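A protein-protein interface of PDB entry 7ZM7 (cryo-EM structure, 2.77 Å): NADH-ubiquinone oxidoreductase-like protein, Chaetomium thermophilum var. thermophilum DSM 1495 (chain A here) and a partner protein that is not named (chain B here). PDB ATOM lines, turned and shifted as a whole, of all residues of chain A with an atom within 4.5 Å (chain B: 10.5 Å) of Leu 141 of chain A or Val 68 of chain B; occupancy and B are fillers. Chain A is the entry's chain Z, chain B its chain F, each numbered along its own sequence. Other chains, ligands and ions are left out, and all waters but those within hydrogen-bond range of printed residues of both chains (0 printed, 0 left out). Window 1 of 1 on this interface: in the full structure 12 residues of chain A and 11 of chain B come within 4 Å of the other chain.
Hydrophobic or aromatic side chains of chain A that line the printed part of chain B: Ala 138, Leu 141, Ala 149 and Leu 153.
Printed residues of chain B that touch a printed residue of chain A: His 66, Val 68, Gln 71, Ser 72, Trp 242, Glu 243 and Pro 244.
Hydrophobic or aromatic side chains of chain B within 4 Å of the printed part of chain A: His 66, Val 68 and Pro 244.
Among the printed residues, 13 pairs touch across the chains.
Among the printed residues, no Asp or Glu carboxylate lies within 4 Å of a Lys or Arg side-chain nitrogen of the other chain.
Among the printed residues, pairs that only touch across the chains: Ala 138 of chain A with Trp 242 of chain B (3.3 Å), Ala 138 of chain A with Glu 243 of chain B (3.7 Å), Ala 138 of chain A with Pro 244 of chain B (3.5 Å), Lys 139 of chain A with Pro 244 of chain B (3.5 Å), Leu 141 of chain A with His 66 of chain B (3.4 Å), Leu 141 of chain A with Val 68 of chain B (3.5 Å), Glu 142 of chain A with His 66 of chain B (3.3 Å), Gly 145 of chain A with His 66 of chain B (3.96 Å), Ala 149 of chain A with His 66 of chain B (3.3 Å), Ala 149 of chain A with Gln 71 of chain B (3.9 Å), Leu 153 of chain A with Val 68 of chain B (3.7 Å), Leu 153 of chain A with Gln 71 of chain B (3.8 Å) and Leu 153 of chain A with Ser 72 of chain B (3.2 Å).
Of chain B, only His 66 (3.4 Å) and Val 68 (3.5 Å) come within 4 Å of Leu 141 of chain A.
Printed residues of chain A within 4 Å of Val 68 of chain B: Leu 141 (3.5 Å) and Leu 153 (3.7 Å).
Printed residues of chain B within 4 Å of Ala 138 of chain A: Trp 242, Glu 243 and Pro 244.
No residue of chain B comes within 4 Å of Tyr 140 of chain A.
Printed residues of chain B within 4 Å of Gly 145 of chain A: His 66 (3.96 Å).
No residue of chain B comes within 4 Å of Glu 148 of chain A.
Ala 149 of chain A touches just these residues of chain B: His 66 (3.3 Å) and Gln 71 (3.9 Å).
Of the printed residues of chain B, Lys 139 of chain A touches Pro 244.
Of the printed residues of chain A, Trp 242 of chain B touches Ala 138.
Of the printed residues of chain A, Ser 72 of chain B touches Leu 153 (3.2 Å).
The backbone carbonyl oxygen of Glu 65 of chain B lies within hydrogen-bond range of the side-chain amide nitrogen of Gln 71 of chain B (2.8 Å).
O of Val 68 of chain B sits at hydrogen-bond distance from OG of Ser 72 of chain B, 3.1 Å away.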
ATOM      1  N   VAL A 137      21.603  16.409 -15.513  1.00  0.00           N
ATOM      2  CA  VAL A 137      22.569  15.825 -16.421  1.00  0.00           C
ATOM      3  C   VAL A 137      22.335  16.345 -17.827  1.00  0.00           C
ATOM      4  O   VAL A 137      23.209  16.219 -18.684  1.00  0.00           O
ATOM      5  CB  VAL A 137      22.528  14.284 -16.371  1.00  0.00           C
ATOM      6  CG1 VAL A 137      22.624  13.794 -14.948  1.00  0.00           C
ATOM      7  CG2 VAL A 137      21.322  13.733 -17.080  1.00  0.00           C
ATOM      8  N   ALA A 138      21.175  16.958 -18.070  1.00  0.00           N
ATOM      9  CA  ALA A 138      20.827  17.433 -19.401  1.00  0.00           C
ATOM     10  C   ALA A 138      21.498  18.758 -19.710  1.00  0.00           C
ATOM     11  O   ALA A 138      22.028  18.946 -20.809  1.00  0.00           O
ATOM     12  CB  ALA A 138      19.315  17.561 -19.534  1.00  0.00           C
ATOM     13  N   LYS A 139      21.446  19.709 -18.774  1.00  0.00           N
ATOM     14  CA  LYS A 139      22.219  20.936 -18.946  1.00  0.00           C
ATOM     15  C   LYS A 139      23.700  20.632 -19.040  1.00  0.00           C
ATOM     16  O   LYS A 139      24.396  21.178 -19.897  1.00  0.00           O
ATOM     17  CB  LYS A 139      21.959  21.911 -17.804  1.00  0.00           C
ATOM     18  CG  LYS A 139      20.549  22.451 -17.702  1.00  0.00           C
ATOM     19  CD  LYS A 139      20.258  23.372 -18.877  1.00  0.00           C
ATOM     20  CE  LYS A 139      18.894  24.024 -18.755  1.00  0.00           C
ATOM     21  NZ  LYS A 139      18.583  24.894 -19.920  1.00  0.00           N
ATOM     22  N   TYR A 140      24.185  19.727 -18.196  1.00  0.00           N
ATOM     23  CA  TYR A 140      25.600  19.392 -18.179  1.00  0.00           C
ATOM     24  C   TYR A 140      26.062  18.835 -19.515  1.00  0.00           C
ATOM     25  O   TYR A 140      27.154  19.158 -19.983  1.00  0.00           O
ATOM     26  CB  TYR A 140      25.867  18.396 -17.054  1.00  0.00           C
ATOM     27  CG  TYR A 140      27.267  17.856 -17.018  1.00  0.00           C
ATOM     28  CD1 TYR A 140      28.304  18.614 -16.517  1.00  0.00           C
ATOM     29  CD2 TYR A 140      27.542  16.586 -17.473  1.00  0.00           C
ATOM     30  CE1 TYR A 140      29.577  18.121 -16.473  1.00  0.00           C
ATOM     31  CE2 TYR A 140      28.816  16.088 -17.441  1.00  0.00           C
ATOM     32  CZ  TYR A 140      29.831  16.860 -16.938  1.00  0.00           C
ATOM     33  OH  TYR A 140      31.106  16.364 -16.902  1.00  0.00           O
ATOM     34  N   LEU A 141      25.253  17.991 -20.146  1.00  0.00           N
ATOM     35  CA  LEU A 141      25.675  17.433 -21.420  1.00  0.00           C
ATOM     36  C   LEU A 141      25.523  18.421 -22.558  1.00  0.00           C
ATOM     37  O   LEU A 141      26.310  18.389 -23.506  1.00  0.00           O
ATOM     38  CB  LEU A 141      24.901  16.158 -21.715  1.00  0.00           C
ATOM     39  CG  LEU A 141      25.239  15.012 -20.762  1.00  0.00           C
ATOM     40  CD1 LEU A 141      24.410  13.808 -21.107  1.00  0.00           C
ATOM     41  CD2 LEU A 141      26.719  14.692 -20.765  1.00  0.00           C
ATOM     42  N   GLU A 142      24.528  19.304 -22.483  1.00  0.00           N
ATOM     43  CA  GLU A 142      24.347  20.310 -23.516  1.00  0.00           C
ATOM     44  C   GLU A 142      25.555  21.228 -23.607  1.00  0.00           C
ATOM     45  O   GLU A 142      26.055  21.505 -24.703  1.00  0.00           O
ATOM     46  CB  GLU A 142      23.085  21.115 -23.230  1.00  0.00           C
ATOM     47  CG  GLU A 142      22.659  22.033 -24.356  1.00  0.00           C
ATOM     48  CD  GLU A 142      23.383  23.362 -24.335  1.00  0.00           C
ATOM     49  OE1 GLU A 142      23.777  23.810 -23.238  1.00  0.00           O
ATOM     50  OE2 GLU A 142      23.574  23.950 -25.418  1.00  0.00           O
ATOM     51  N   GLU A 143      26.055  21.692 -22.461  1.00  0.00           N
ATOM     52  CA  GLU A 143      26.991  22.806 -22.475  1.00  0.00           C
ATOM     53  C   GLU A 143      28.437  22.368 -22.655  1.00  0.00           C
ATOM     54  O   GLU A 143      29.227  23.114 -23.243  1.00  0.00           O
ATOM     55  CB  GLU A 143      26.846  23.635 -21.199  1.00  0.00           C
ATOM     56  CG  GLU A 143      26.848  22.828 -19.922  1.00  0.00           C
ATOM     57  CD  GLU A 143      28.228  22.555 -19.397  1.00  0.00           C
ATOM     58  OE1 GLU A 143      29.175  23.243 -19.828  1.00  0.00           O
ATOM     59  OE2 GLU A 143      28.363  21.649 -18.551  1.00  0.00           O
ATOM     60  N   LYS A 144      28.813  21.190 -22.172  1.00  0.00           N
ATOM     61  CA  LYS A 144      30.162  20.705 -22.411  1.00  0.00           C
ATOM     62  C   LYS A 144      30.275  19.940 -23.714  1.00  0.00           C
ATOM     63  O   LYS A 144      31.327  19.356 -23.987  1.00  0.00           O
ATOM     64  CB  LYS A 144      30.648  19.831 -21.265  1.00  0.00           C
ATOM     65  CG  LYS A 144      30.897  20.555 -19.973  1.00  0.00           C
ATOM     66  CD  LYS A 144      31.323  19.589 -18.899  1.00  0.00           C
ATOM     67  CE  LYS A 144      32.724  19.072 -19.158  1.00  0.00           C
ATOM     68  NZ  LYS A 144      33.734  20.156 -19.003  1.00  0.00           N
ATOM     69  N   GLY A 145      29.210  19.902 -24.500  1.00  0.00           N
ATOM     70  CA  GLY A 145      29.271  19.450 -25.872  1.00  0.00           C
ATOM     71  C   GLY A 145      29.121  17.948 -26.004  1.00  0.00           C
ATOM     72  O   GLY A 145      29.160  17.188 -25.036  1.00  0.00           O
ATOM     73  N   GLU A 148      31.508  14.913 -24.426  1.00  0.00           N
ATOM     74  CA  GLU A 148      31.266  14.095 -23.247  1.00  0.00           C
ATOM     75  C   GLU A 148      29.966  13.310 -23.336  1.00  0.00           C
ATOM     76  O   GLU A 148      29.625  12.606 -22.385  1.00  0.00           O
ATOM     77  CB  GLU A 148      31.239  14.922 -21.972  1.00  0.00           C
ATOM     78  CG  GLU A 148      30.090  15.864 -21.889  1.00  0.00           C
ATOM     79  CD  GLU A 148      30.136  16.657 -20.630  1.00  0.00           C
ATOM     80  OE1 GLU A 148      31.095  16.462 -19.862  1.00  0.00           O
ATOM     81  OE2 GLU A 148      29.189  17.424 -20.383  1.00  0.00           O
ATOM     82  N   ALA A 149      29.205  13.459 -24.418  1.00  0.00           N
ATOM     83  CA  ALA A 149      28.205  12.452 -24.739  1.00  0.00           C
ATOM     84  C   ALA A 149      28.867  11.165 -25.205  1.00  0.00           C
ATOM     85  O   ALA A 149      28.316  10.075 -25.014  1.00  0.00           O
ATOM     86  CB  ALA A 149      27.253  12.969 -25.812  1.00  0.00           C
ATOM     87  N   VAL A 152      30.141   9.242 -21.849  1.00  0.00           N
ATOM     88  CA  VAL A 152      29.212   8.404 -21.107  1.00  0.00           C
ATOM     89  C   VAL A 152      29.238   6.982 -21.650  1.00  0.00           C
ATOM     90  O   VAL A 152      29.137   6.010 -20.892  1.00  0.00           O
ATOM     91  CB  VAL A 152      27.801   9.011 -21.157  1.00  0.00           C
ATOM     92  CG1 VAL A 152      26.866   8.226 -20.280  1.00  0.00           C
ATOM     93  CG2 VAL A 152      27.840  10.444 -20.726  1.00  0.00           C
ATOM     94  N   LEU A 153      29.368   6.831 -22.966  1.00  0.00           N
ATOM     95  CA  LEU A 153      29.549   5.501 -23.530  1.00  0.00           C
ATOM     96  C   LEU A 153      30.972   4.984 -23.362  1.00  0.00           C
ATOM     97  O   LEU A 153      31.188   3.772 -23.361  1.00  0.00           O
ATOM     98  CB  LEU A 153      29.168   5.493 -25.008  1.00  0.00           C
ATOM     99  CG  LEU A 153      27.769   4.995 -25.325  1.00  0.00           C
ATOM    100  CD1 LEU A 153      26.759   5.990 -24.864  1.00  0.00           C
ATOM    101  CD2 LEU A 153      27.666   4.805 -26.792  1.00  0.00           C
ATOM    102  N   LEU B  60      17.945  10.113 -36.835  1.00  0.00           N
ATOM    103  CA  LEU B  60      18.732  10.531 -35.690  1.00  0.00           C
ATOM    104  C   LEU B  60      19.318  11.921 -35.854  1.00  0.00           C
ATOM    105  O   LEU B  60      19.894  12.450 -34.902  1.00  0.00           O
ATOM    106  CB  LEU B  60      19.851   9.526 -35.436  1.00  0.00           C
ATOM    107  CG  LEU B  60      19.371   8.200 -34.844  1.00  0.00           C
ATOM    108  CD1 LEU B  60      20.536   7.265 -34.683  1.00  0.00           C
ATOM    109  CD2 LEU B  60      18.652   8.395 -33.523  1.00  0.00           C
ATOM    110  N   ILE B  63      17.864  14.809 -33.803  1.00  0.00           N
ATOM    111  CA  ILE B  63      18.250  14.822 -32.399  1.00  0.00           C
ATOM    112  C   ILE B  63      19.609  15.494 -32.283  1.00  0.00           C
ATOM    113  O   ILE B  63      20.472  15.279 -33.144  1.00  0.00           O
ATOM    114  CB  ILE B  63      18.275  13.399 -31.825  1.00  0.00           C
ATOM    115  CG1 ILE B  63      16.888  12.798 -31.868  1.00  0.00           C
ATOM    116  CG2 ILE B  63      18.771  13.387 -30.425  1.00  0.00           C
ATOM    117  CD1 ILE B  63      16.870  11.341 -31.599  1.00  0.00           C
ATOM    118  N   PRO B  64      19.841  16.309 -31.257  1.00  0.00           N
ATOM    119  CA  PRO B  64      21.135  16.974 -31.115  1.00  0.00           C
ATOM    120  C   PRO B  64      22.267  15.989 -30.908  1.00  0.00           C
ATOM    121  O   PRO B  64      22.063  14.810 -30.620  1.00  0.00           O
ATOM    122  CB  PRO B  64      20.940  17.857 -29.888  1.00  0.00           C
ATOM    123  CG  PRO B  64      19.495  18.088 -29.834  1.00  0.00           C
ATOM    124  CD  PRO B  64      18.846  16.855 -30.327  1.00  0.00           C
ATOM    125  N   GLU B  65      23.486  16.488 -31.087  1.00  0.00           N
ATOM    126  CA  GLU B  65      24.661  15.635 -31.005  1.00  0.00           C
ATOM    127  C   GLU B  65      25.014  15.241 -29.581  1.00  0.00           C
ATOM    128  O   GLU B  65      25.616  14.186 -29.382  1.00  0.00           O
ATOM    129  CB  GLU B  65      25.854  16.328 -31.649  1.00  0.00           C
ATOM    130  CG  GLU B  65      25.718  16.537 -33.142  1.00  0.00           C
ATOM    131  CD  GLU B  65      25.714  15.233 -33.913  1.00  0.00           C
ATOM    132  OE1 GLU B  65      26.375  14.272 -33.469  1.00  0.00           O
ATOM    133  OE2 GLU B  65      25.052  15.170 -34.967  1.00  0.00           O
ATOM    134  N   HIS B  66      24.662  16.047 -28.592  1.00  0.00           N
ATOM    135  CA  HIS B  66      25.107  15.803 -27.233  1.00  0.00           C
ATOM    136  C   HIS B  66      24.192  14.869 -26.457  1.00  0.00           C
ATOM    137  O   HIS B  66      24.465  14.596 -25.289  1.00  0.00           O
ATOM    138  CB  HIS B  66      25.272  17.126 -26.471  1.00  0.00           C
ATOM    139  CG  HIS B  66      24.015  17.917 -26.335  1.00  0.00           C
ATOM    140  ND1 HIS B  66      23.639  18.877 -27.243  1.00  0.00           N
ATOM    141  CD2 HIS B  66      23.036  17.880 -25.404  1.00  0.00           C
ATOM    142  CE1 HIS B  66      22.494  19.415 -26.867  1.00  0.00           C
ATOM    143  NE2 HIS B  66      22.100  18.816 -25.761  1.00  0.00           N
ATOM    144  N   SER B  67      23.131  14.363 -27.070  1.00  0.00           N
ATOM    145  CA  SER B  67      22.267  13.415 -26.396  1.00  0.00           C
ATOM    146  C   SER B  67      22.901  12.038 -26.436  1.00  0.00           C
ATOM    147  O   SER B  67      23.200  11.507 -27.507  1.00  0.00           O
ATOM    148  CB  SER B  67      20.886  13.354 -27.031  1.00  0.00           C
ATOM    149  OG  SER B  67      20.959  12.754 -28.289  1.00  0.00           O
ATOM    150  N   VAL B  68      23.062  11.455 -25.254  1.00  0.00           N
ATOM    151  CA  VAL B  68      23.564  10.099 -25.121  1.00  0.00           C
ATOM    152  C   VAL B  68      22.648   9.100 -25.810  1.00  0.00           C
ATOM    153  O   VAL B  68      23.101   8.039 -26.246  1.00  0.00           O
ATOM    154  CB  VAL B  68      23.743   9.791 -23.626  1.00  0.00           C
ATOM    155  CG1 VAL B  68      24.389   8.444 -23.427  1.00  0.00           C
ATOM    156  CG2 VAL B  68      24.573  10.870 -23.000  1.00  0.00           C
ATOM    157  N   TYR B  69      21.357   9.409 -25.929  1.00  0.00           N
ATOM    158  CA  TYR B  69      20.467   8.503 -26.640  1.00  0.00           C
ATOM    159  C   TYR B  69      20.915   8.325 -28.082  1.00  0.00           C
ATOM    160  O   TYR B  69      21.072   7.201 -28.563  1.00  0.00           O
ATOM    161  CB  TYR B  69      19.031   9.017 -26.575  1.00  0.00           C
ATOM    162  CG  TYR B  69      18.119   8.369 -27.583  1.00  0.00           C
ATOM    163  CD1 TYR B  69      17.557   7.136 -27.342  1.00  0.00           C
ATOM    164  CD2 TYR B  69      17.845   8.983 -28.785  1.00  0.00           C
ATOM    165  CE1 TYR B  69      16.747   6.541 -28.269  1.00  0.00           C
ATOM    166  CE2 TYR B  69      17.048   8.396 -29.713  1.00  0.00           C
ATOM    167  CZ  TYR B  69      16.498   7.179 -29.457  1.00  0.00           C
ATOM    168  OH  TYR B  69      15.683   6.597 -30.387  1.00  0.00           O
ATOM    169  N   ARG B  70      21.150   9.431 -28.783  1.00  0.00           N
ATOM    170  CA  ARG B  70      21.567   9.369 -30.177  1.00  0.00           C
ATOM    171  C   ARG B  70      22.912   8.674 -30.325  1.00  0.00           C
ATOM    172  O   ARG B  70      23.095   7.852 -31.222  1.00  0.00           O
ATOM    173  CB  ARG B  70      21.615  10.782 -30.744  1.00  0.00           C
ATOM    174  CG  ARG B  70      21.784  10.921 -32.235  1.00  0.00           C
ATOM    175  CD  ARG B  70      22.072  12.375 -32.516  1.00  0.00           C
ATOM    176  NE  ARG B  70      22.116  12.718 -33.929  1.00  0.00           N
ATOM    177  CZ  ARG B  70      23.216  12.703 -34.665  1.00  0.00           C
ATOM    178  NH1 ARG B  70      24.371  12.356 -34.122  1.00  0.00           N
ATOM    179  NH2 ARG B  70      23.157  13.034 -35.943  1.00  0.00           N
ATOM    180  N   GLN B  71      23.863   8.982 -29.447  1.00  0.00           N
ATOM    181  CA  GLN B  71      25.162   8.319 -29.485  1.00  0.00           C
ATOM    182  C   GLN B  71      25.032   6.830 -29.239  1.00  0.00           C
ATOM    183  O   GLN B  71      25.736   6.028 -29.855  1.00  0.00           O
ATOM    184  CB  GLN B  71      26.081   8.929 -28.441  1.00  0.00           C
ATOM    185  CG  GLN B  71      26.092  10.414 -28.451  1.00  0.00           C
ATOM    186  CD  GLN B  71      27.260  10.937 -29.196  1.00  0.00           C
ATOM    187  OE1 GLN B  71      28.375  10.498 -28.972  1.00  0.00           O
ATOM    188  NE2 GLN B  71      27.019  11.859 -30.120  1.00  0.00           N
ATOM    189  N   SER B  72      24.163   6.445 -28.305  1.00  0.00           N
ATOM    190  CA  SER B  72      23.932   5.032 -28.024  1.00  0.00           C
ATOM    191  C   SER B  72      23.302   4.328 -29.212  1.00  0.00           C
ATOM    192  O   SER B  72      23.755   3.258 -29.625  1.00  0.00           O
ATOM    193  CB  SER B  72      23.041   4.889 -26.801  1.00  0.00           C
ATOM    194  OG  SER B  72      23.794   5.081 -25.633  1.00  0.00           O
ATOM    195  N   VAL B  73      22.258   4.923 -29.777  1.00  0.00           N
ATOM    196  CA  VAL B  73      21.601   4.329 -30.930  1.00  0.00           C
ATOM    197  C   VAL B  73      22.519   4.366 -32.146  1.00  0.00           C
ATOM    198  O   VAL B  73      22.605   3.391 -32.896  1.00  0.00           O
ATOM    199  CB  VAL B  73      20.258   5.033 -31.195  1.00  0.00           C
ATOM    200  CG1 VAL B  73      19.576   4.454 -32.415  1.00  0.00           C
ATOM    201  CG2 VAL B  73      19.366   4.912 -30.005  1.00  0.00           C
ATOM    202  N   GLU B  74      23.233   5.476 -32.354  1.00  0.00           N
ATOM    203  CA  GLU B  74      24.144   5.567 -33.493  1.00  0.00           C
ATOM    204  C   GLU B  74      25.215   4.496 -33.445  1.00  0.00           C
ATOM    205  O   GLU B  74      25.434   3.785 -34.429  1.00  0.00           O
ATOM    206  CB  GLU B  74      24.813   6.934 -33.558  1.00  0.00           C
ATOM    207  CG  GLU B  74      24.096   7.970 -34.356  1.00  0.00           C
ATOM    208  CD  GLU B  74      24.935   9.212 -34.520  1.00  0.00           C
ATOM    209  OE1 GLU B  74      26.003   9.290 -33.883  1.00  0.00           O
ATOM    210  OE2 GLU B  74      24.543  10.105 -35.298  1.00  0.00           O
ATOM    211  N   ALA B  75      25.916   4.385 -32.318  1.00  0.00           N
ATOM    212  CA  ALA B  75      27.023   3.441 -32.237  1.00  0.00           C
ATOM    213  C   ALA B  75      26.547   2.020 -32.432  1.00  0.00           C
ATOM    214  O   ALA B  75      27.166   1.248 -33.172  1.00  0.00           O
ATOM    215  CB  ALA B  75      27.740   3.569 -30.901  1.00  0.00           C
ATOM    216  N   VAL B  76      25.455   1.650 -31.771  1.00  0.00           N
ATOM    217  CA  VAL B  76      24.943   0.292 -31.882  1.00  0.00           C
ATOM    218  C   VAL B  76      24.479   0.028 -33.302  1.00  0.00           C
ATOM    219  O   VAL B  76      24.775  -1.020 -33.878  1.00  0.00           O
ATOM    220  CB  VAL B  76      23.817   0.061 -30.854  1.00  0.00           C
ATOM    221  CG1 VAL B  76      22.995  -1.154 -31.194  1.00  0.00           C
ATOM    222  CG2 VAL B  76      24.395  -0.120 -29.486  1.00  0.00           C
ATOM    223  N   THR B  77      23.746   0.978 -33.884  1.00  0.00           N
ATOM    224  CA  THR B  77      23.223   0.806 -35.233  1.00  0.00           C
ATOM    225  C   THR B  77      24.344   0.695 -36.249  1.00  0.00           C
ATOM    226  O   THR B  77      24.278  -0.125 -37.167  1.00  0.00           O
ATOM    227  CB  THR B  77      22.313   1.972 -35.595  1.00  0.00           C
ATOM    228  OG1 THR B  77      21.336   2.147 -34.566  1.00  0.00           O
ATOM    229  CG2 THR B  77      21.612   1.708 -36.914  1.00  0.00           C
ATOM    230  N   GLU B 229      13.689  -0.196 -33.179  1.00  0.00           N
ATOM    231  CA  GLU B 229      14.537   0.979 -33.018  1.00  0.00           C
ATOM    232  C   GLU B 229      14.123   2.090 -33.971  1.00  0.00           C
ATOM    233  O   GLU B 229      14.247   3.274 -33.649  1.00  0.00           O
ATOM    234  CB  GLU B 229      16.007   0.604 -33.220  1.00  0.00           C
ATOM    235  CG  GLU B 229      17.009   1.643 -32.692  1.00  0.00           C
ATOM    236  CD  GLU B 229      16.945   1.845 -31.149  1.00  0.00           C
ATOM    237  OE1 GLU B 229      17.876   1.412 -30.430  1.00  0.00           O
ATOM    238  OE2 GLU B 229      15.972   2.458 -30.662  1.00  0.00           O
ATOM    239  N   MET B 236      11.097   9.436 -29.448  1.00  0.00           N
ATOM    240  CA  MET B 236      12.187  10.107 -28.749  1.00  0.00           C
ATOM    241  C   MET B 236      12.390  11.536 -29.225  1.00  0.00           C
ATOM    242  O   MET B 236      12.899  12.364 -28.464  1.00  0.00           O
ATOM    243  CB  MET B 236      13.481   9.301 -28.879  1.00  0.00           C
ATOM    244  CG  MET B 236      13.540   8.019 -28.035  1.00  0.00           C
ATOM    245  SD  MET B 236      13.054   8.274 -26.317  1.00  0.00           S
ATOM    246  CE  MET B 236      11.422   7.581 -26.246  1.00  0.00           C
ATOM    247  N   ARG B 240      11.423  14.905 -26.800  1.00  0.00           N
ATOM    248  CA  ARG B 240      12.635  15.684 -26.539  1.00  0.00           C
ATOM    249  C   ARG B 240      13.311  15.240 -25.247  1.00  0.00           C
ATOM    250  O   ARG B 240      13.557  16.021 -24.337  1.00  0.00           O
ATOM    251  CB  ARG B 240      12.337  17.184 -26.509  1.00  0.00           C
ATOM    252  CG  ARG B 240      11.498  17.653 -27.652  1.00  0.00           C
ATOM    253  CD  ARG B 240      11.457  19.163 -27.724  1.00  0.00           C
ATOM    254  NE  ARG B 240      12.788  19.751 -27.831  1.00  0.00           N
ATOM    255  CZ  ARG B 240      13.468  19.861 -28.964  1.00  0.00           C
ATOM    256  NH1 ARG B 240      14.672  20.411 -28.962  1.00  0.00           N
ATOM    257  NH2 ARG B 240      12.944  19.423 -30.099  1.00  0.00           N
ATOM    258  N   VAL B 241      13.652  13.955 -25.209  1.00  0.00           N
ATOM    259  CA  VAL B 241      14.080  13.337 -23.971  1.00  0.00           C
ATOM    260  C   VAL B 241      15.396  13.906 -23.468  1.00  0.00           C
ATOM    261  O   VAL B 241      15.740  13.713 -22.300  1.00  0.00           O
ATOM    262  CB  VAL B 241      14.133  11.807 -24.160  1.00  0.00           C
ATOM    263  CG1 VAL B 241      12.748  11.285 -24.430  1.00  0.00           C
ATOM    264  CG2 VAL B 241      15.054  11.432 -25.292  1.00  0.00           C
ATOM    265  N   TRP B 242      16.133  14.624 -24.315  1.00  0.00           N
ATOM    266  CA  TRP B 242      17.403  15.235 -23.944  1.00  0.00           C
ATOM    267  C   TRP B 242      17.248  16.553 -23.192  1.00  0.00           C
ATOM    268  O   TRP B 242      18.223  17.044 -22.624  1.00  0.00           O
ATOM    269  CB  TRP B 242      18.228  15.460 -25.204  1.00  0.00           C
ATOM    270  CG  TRP B 242      17.482  16.245 -26.232  1.00  0.00           C
ATOM    271  CD1 TRP B 242      17.373  17.601 -26.309  1.00  0.00           C
ATOM    272  CD2 TRP B 242      16.727  15.723 -27.321  1.00  0.00           C
ATOM    273  NE1 TRP B 242      16.599  17.955 -27.380  1.00  0.00           N
ATOM    274  CE2 TRP B 242      16.188  16.818 -28.018  1.00  0.00           C
ATOM    275  CE3 TRP B 242      16.459  14.436 -27.782  1.00  0.00           C
ATOM    276  CZ2 TRP B 242      15.400  16.662 -29.148  1.00  0.00           C
ATOM    277  CZ3 TRP B 242      15.676  14.287 -28.896  1.00  0.00           C
ATOM    278  CH2 TRP B 242      15.163  15.386 -29.571  1.00  0.00           C
ATOM    279  N   GLU B 243      16.060  17.134 -23.188  1.00  0.00           N
ATOM    280  CA  GLU B 243      15.782  18.360 -22.463  1.00  0.00           C
ATOM    281  C   GLU B 243      15.877  18.119 -20.951  1.00  0.00           C
ATOM    282  O   GLU B 243      15.741  16.987 -20.491  1.00  0.00           O
ATOM    283  CB  GLU B 243      14.388  18.850 -22.844  1.00  0.00           C
ATOM    284  CG  GLU B 243      14.089  20.331 -22.651  1.00  0.00           C
ATOM    285  CD  GLU B 243      13.533  20.649 -21.271  1.00  0.00           C
ATOM    286  OE1 GLU B 243      12.795  19.818 -20.711  1.00  0.00           O
ATOM    287  OE2 GLU B 243      13.851  21.733 -20.742  1.00  0.00           O
ATOM    288  N   PRO B 244      16.144  19.160 -20.162  1.00  0.00           N
ATOM    289  CA  PRO B 244      16.235  19.000 -18.704  1.00  0.00           C
ATOM    290  C   PRO B 244      15.011  18.360 -18.059  1.00  0.00           C
ATOM    291  O   PRO B 244      13.923  18.284 -18.625  1.00  0.00           O
ATOM    292  CB  PRO B 244      16.413  20.440 -18.229  1.00  0.00           C
ATOM    293  CG  PRO B 244      17.138  21.070 -19.313  1.00  0.00           C
ATOM    294  CD  PRO B 244      16.727  20.439 -20.585  1.00  0.00           C
